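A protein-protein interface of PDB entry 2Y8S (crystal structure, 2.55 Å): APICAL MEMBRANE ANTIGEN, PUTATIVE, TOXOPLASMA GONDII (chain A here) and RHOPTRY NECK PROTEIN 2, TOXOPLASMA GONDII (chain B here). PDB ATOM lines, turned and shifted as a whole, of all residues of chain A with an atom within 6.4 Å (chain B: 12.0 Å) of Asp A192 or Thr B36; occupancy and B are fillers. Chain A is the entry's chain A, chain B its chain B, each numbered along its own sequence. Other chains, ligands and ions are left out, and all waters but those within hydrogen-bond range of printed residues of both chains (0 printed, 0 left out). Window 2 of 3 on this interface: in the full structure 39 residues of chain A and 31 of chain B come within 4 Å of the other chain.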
ATOM      1  N   TYR A  90      13.570 -26.637  -9.212  1.00  0.00           N
ATOM      2  CA  TYR A  90      14.232 -26.789  -7.921  1.00  0.00           C
ATOM      3  C   TYR A  90      15.002 -28.109  -7.858  1.00  0.00           C
ATOM      4  O   TYR A  90      16.148 -28.158  -7.371  1.00  0.00           O
ATOM      5  CB  TYR A  90      13.162 -26.722  -6.861  1.00  0.00           C
ATOM      6  CG  TYR A  90      13.600 -26.766  -5.445  1.00  0.00           C
ATOM      7  CD1 TYR A  90      14.738 -26.108  -5.014  1.00  0.00           C
ATOM      8  CD2 TYR A  90      12.834 -27.440  -4.514  1.00  0.00           C
ATOM      9  CE1 TYR A  90      15.118 -26.143  -3.715  1.00  0.00           C
ATOM     10  CE2 TYR A  90      13.197 -27.469  -3.185  1.00  0.00           C
ATOM     11  CZ  TYR A  90      14.345 -26.820  -2.790  1.00  0.00           C
ATOM     12  OH  TYR A  90      14.698 -26.866  -1.459  1.00  0.00           O
ATOM     13  N   ASN A  95      19.452 -26.585  -3.305  1.00  0.00           N
ATOM     14  CA  ASN A  95      19.181 -25.425  -2.508  1.00  0.00           C
ATOM     15  C   ASN A  95      20.183 -24.347  -2.825  1.00  0.00           C
ATOM     16  O   ASN A  95      21.315 -24.680  -3.131  1.00  0.00           O
ATOM     17  CB  ASN A  95      19.314 -25.797  -1.063  1.00  0.00           C
ATOM     18  CG  ASN A  95      18.092 -26.463  -0.538  1.00  0.00           C
ATOM     19  OD1 ASN A  95      18.179 -27.275   0.360  1.00  0.00           O
ATOM     20  ND2 ASN A  95      16.935 -26.118  -1.072  1.00  0.00           N
ATOM     21  N   GLY A 188      24.844 -19.016  -1.557  1.00  0.00           N
ATOM     22  CA  GLY A 188      24.984 -20.458  -1.354  1.00  0.00           C
ATOM     23  C   GLY A 188      25.653 -20.917  -0.061  1.00  0.00           C
ATOM     24  O   GLY A 188      25.929 -22.099   0.092  1.00  0.00           O
ATOM     25  N   PRO A 190      25.421 -21.007   4.161  1.00  0.00           N
ATOM     26  CA  PRO A 190      25.611 -22.483   4.177  1.00  0.00           C
ATOM     27  C   PRO A 190      24.871 -23.165   3.029  1.00  0.00           C
ATOM     28  O   PRO A 190      23.981 -22.555   2.452  1.00  0.00           O
ATOM     29  CB  PRO A 190      24.952 -22.915   5.497  1.00  0.00           C
ATOM     30  CG  PRO A 190      24.891 -21.672   6.333  1.00  0.00           C
ATOM     31  CD  PRO A 190      24.711 -20.541   5.370  1.00  0.00           C
ATOM     32  N   PRO A 191      25.231 -24.417   2.689  1.00  0.00           N
ATOM     33  CA  PRO A 191      24.636 -25.061   1.488  1.00  0.00           C
ATOM     34  C   PRO A 191      23.281 -25.840   1.595  1.00  0.00           C
ATOM     35  O   PRO A 191      22.569 -26.010   0.597  1.00  0.00           O
ATOM     36  CB  PRO A 191      25.767 -25.976   0.989  1.00  0.00           C
ATOM     37  CG  PRO A 191      26.607 -26.232   2.192  1.00  0.00           C
ATOM     38  CD  PRO A 191      26.525 -25.024   3.065  1.00  0.00           C
ATOM     39  N   ASP A 192      22.924 -26.301   2.781  1.00  0.00           N
ATOM     40  CA  ASP A 192      21.714 -27.115   2.951  1.00  0.00           C
ATOM     41  C   ASP A 192      20.434 -26.271   3.030  1.00  0.00           C
ATOM     42  O   ASP A 192      19.321 -26.819   3.120  1.00  0.00           O
ATOM     43  CB  ASP A 192      21.839 -27.920   4.244  1.00  0.00           C
ATOM     44  CG  ASP A 192      22.259 -27.038   5.435  1.00  0.00           C
ATOM     45  OD1 ASP A 192      23.365 -26.435   5.361  1.00  0.00           O
ATOM     46  OD2 ASP A 192      21.479 -26.946   6.423  1.00  0.00           O
ATOM     47  N   LEU A 193      20.590 -24.948   3.011  1.00  0.00           N
ATOM     48  CA  LEU A 193      19.457 -24.041   3.247  1.00  0.00           C
ATOM     49  C   LEU A 193      18.520 -23.873   2.058  1.00  0.00           C
ATOM     50  O   LEU A 193      18.942 -23.766   0.892  1.00  0.00           O
ATOM     51  CB  LEU A 193      19.919 -22.678   3.778  1.00  0.00           C
ATOM     52  CG  LEU A 193      20.549 -22.756   5.172  1.00  0.00           C
ATOM     53  CD1 LEU A 193      21.142 -21.418   5.582  1.00  0.00           C
ATOM     54  CD2 LEU A 193      19.549 -23.288   6.213  1.00  0.00           C
ATOM     55  N   THR A 194      17.240 -23.844   2.398  1.00  0.00           N
ATOM     56  CA  THR A 194      16.156 -23.747   1.447  1.00  0.00           C
ATOM     57  C   THR A 194      16.129 -22.381   0.790  1.00  0.00           C
ATOM     58  O   THR A 194      16.097 -22.262  -0.421  1.00  0.00           O
ATOM     59  CB  THR A 194      14.855 -23.959   2.182  1.00  0.00           C
ATOM     60  OG1 THR A 194      15.039 -25.049   3.083  1.00  0.00           O
ATOM     61  CG2 THR A 194      13.737 -24.291   1.232  1.00  0.00           C
ATOM     62  N   ILE B   2       9.027 -23.239  12.375  1.00  0.00           N
ATOM     63  CA  ILE B   2       9.383 -22.621  11.131  1.00  0.00           C
ATOM     64  C   ILE B   2       8.180 -21.952  10.449  1.00  0.00           C
ATOM     65  O   ILE B   2       8.342 -20.915   9.799  1.00  0.00           O
ATOM     66  CB  ILE B   2      10.127 -23.641  10.193  1.00  0.00           C
ATOM     67  CG1 ILE B   2      10.560 -22.972   8.881  1.00  0.00           C
ATOM     68  CG2 ILE B   2       9.328 -24.927   9.976  1.00  0.00           C
ATOM     69  CD1 ILE B   2      11.593 -21.832   9.093  1.00  0.00           C
ATOM     70  N   MET B   6       7.929 -18.093   9.367  1.00  0.00           N
ATOM     71  CA  MET B   6       7.564 -17.711   8.004  1.00  0.00           C
ATOM     72  C   MET B   6       6.363 -16.765   7.941  1.00  0.00           C
ATOM     73  O   MET B   6       6.422 -15.734   7.291  1.00  0.00           O
ATOM     74  CB  MET B   6       7.313 -18.943   7.136  1.00  0.00           C
ATOM     75  CG  MET B   6       8.560 -19.766   6.890  1.00  0.00           C
ATOM     76  SD  MET B   6       9.793 -18.788   6.034  1.00  0.00           S
ATOM     77  CE  MET B   6      11.339 -19.449   6.685  1.00  0.00           C
ATOM     78  N   ILE B  32       4.279 -26.295  -8.024  1.00  0.00           N
ATOM     79  CA  ILE B  32       5.148 -25.262  -7.469  1.00  0.00           C
ATOM     80  C   ILE B  32       6.127 -25.885  -6.502  1.00  0.00           C
ATOM     81  O   ILE B  32       5.746 -26.750  -5.719  1.00  0.00           O
ATOM     82  CB  ILE B  32       4.321 -24.141  -6.766  1.00  0.00           C
ATOM     83  CG1 ILE B  32       3.676 -23.212  -7.800  1.00  0.00           C
ATOM     84  CG2 ILE B  32       5.197 -23.276  -5.805  1.00  0.00           C
ATOM     85  CD1 ILE B  32       4.669 -22.228  -8.499  1.00  0.00           C
ATOM     86  N   ALA B  33       7.384 -25.458  -6.559  1.00  0.00           N
ATOM     87  CA  ALA B  33       8.437 -25.941  -5.656  1.00  0.00           C
ATOM     88  C   ALA B  33       8.083 -25.812  -4.162  1.00  0.00           C
ATOM     89  O   ALA B  33       7.570 -24.768  -3.731  1.00  0.00           O
ATOM     90  CB  ALA B  33       9.758 -25.234  -5.970  1.00  0.00           C
ATOM     91  N   LYS B  34       8.367 -26.862  -3.380  1.00  0.00           N
ATOM     92  CA  LYS B  34       7.950 -26.891  -1.967  1.00  0.00           C
ATOM     93  C   LYS B  34       9.043 -26.737  -0.876  1.00  0.00           C
ATOM     94  O   LYS B  34       9.119 -25.652  -0.267  1.00  0.00           O
ATOM     95  CB  LYS B  34       6.992 -28.064  -1.680  1.00  0.00           C
ATOM     96  CG  LYS B  34       5.778 -28.179  -2.642  1.00  0.00           C
ATOM     97  CD  LYS B  34       5.298 -29.638  -2.753  1.00  0.00           C
ATOM     98  CE  LYS B  34       5.332 -30.184  -4.203  1.00  0.00           C
ATOM     99  NZ  LYS B  34       4.025 -30.195  -4.946  1.00  0.00           N
ATOM    100  N   ALA B  35       9.876 -27.756  -0.601  1.00  0.00           N
ATOM    101  CA  ALA B  35      10.714 -27.733   0.667  1.00  0.00           C
ATOM    102  C   ALA B  35      12.108 -28.434   0.653  1.00  0.00           C
ATOM    103  O   ALA B  35      12.650 -28.714  -0.409  1.00  0.00           O
ATOM    104  CB  ALA B  35       9.866 -28.217   1.889  1.00  0.00           C
ATOM    105  N   THR B  36      12.685 -28.677   1.834  1.00  0.00           N
ATOM    106  CA  THR B  36      13.934 -29.457   2.014  1.00  0.00           C
ATOM    107  C   THR B  36      13.935 -30.117   3.373  1.00  0.00           C
ATOM    108  O   THR B  36      14.685 -29.701   4.265  1.00  0.00           O
ATOM    109  CB  THR B  36      15.229 -28.592   1.966  1.00  0.00           C
ATOM    110  OG1 THR B  36      15.433 -28.083   0.643  1.00  0.00           O
ATOM    111  CG2 THR B  36      16.487 -29.410   2.413  1.00  0.00           C
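The side-chain hydroxyl of Tyr A90 lies within hydrogen-bond range of the backbone carbonyl oxygen of Ala B35, 3.0 Å away. The side-chain hydroxyl (OH) of Tyr A90 lies within hydrogen-bond range of the side-chain hydroxyl (OG1) of Thr B36. The side-chain amide oxygen (OD1) of Asn A95 lies within hydrogen-bond range of the side-chain hydroxyl (OG1) of Thr B36.
OD1 of Asn A95 lies close to O of Asp A192, at 3.0 Å.
Printed residues of chain B within 4 Å of Tyr A90: Ala B33 (3.8 Å), Ala B35 (3.0 Å) and Thr B36 (2.5 Å). Of chain B, only Thr B36 (2.9 Å) comes within 4 Å of Asn A95. No residue of chain B comes within 4 Å of Pro A190. No residue of chain B comes within 4 Å of Pro A191. Of chain B, only Thr B36 (3.9 Å) comes within 4 Å of Asp A192. No residue of chain B comes within 4 Å of Leu A193. Of chain B, only Thr B36 (3.7 Å) comes within 4 Å of Thr A194. Of the printed residues of chain A, Ala B33 touches Tyr A90 (3.8 Å). Printed residues of chain A within 4 Å of Ala B35: Tyr A90.
Among the printed residues, pairs that only touch across the chains: Tyr A90 with Ala B33, Asp A192 with Thr B36 and Thr A194 with Thr B36.
Hydrophobic or aromatic side chains of chain B within 4 Å of the printed part of chain A: Ala B33. Printed residues of chain A that touch a printed residue of chain B: Tyr A90, Asn A95, Asp A192 and Thr A194. Among the printed residues, 6 pairs touch across the chains. Among the printed residues, no Asp or Glu carboxylate lies within 4 Å of a Lys or Arg side-chain nitrogen of the other chain.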
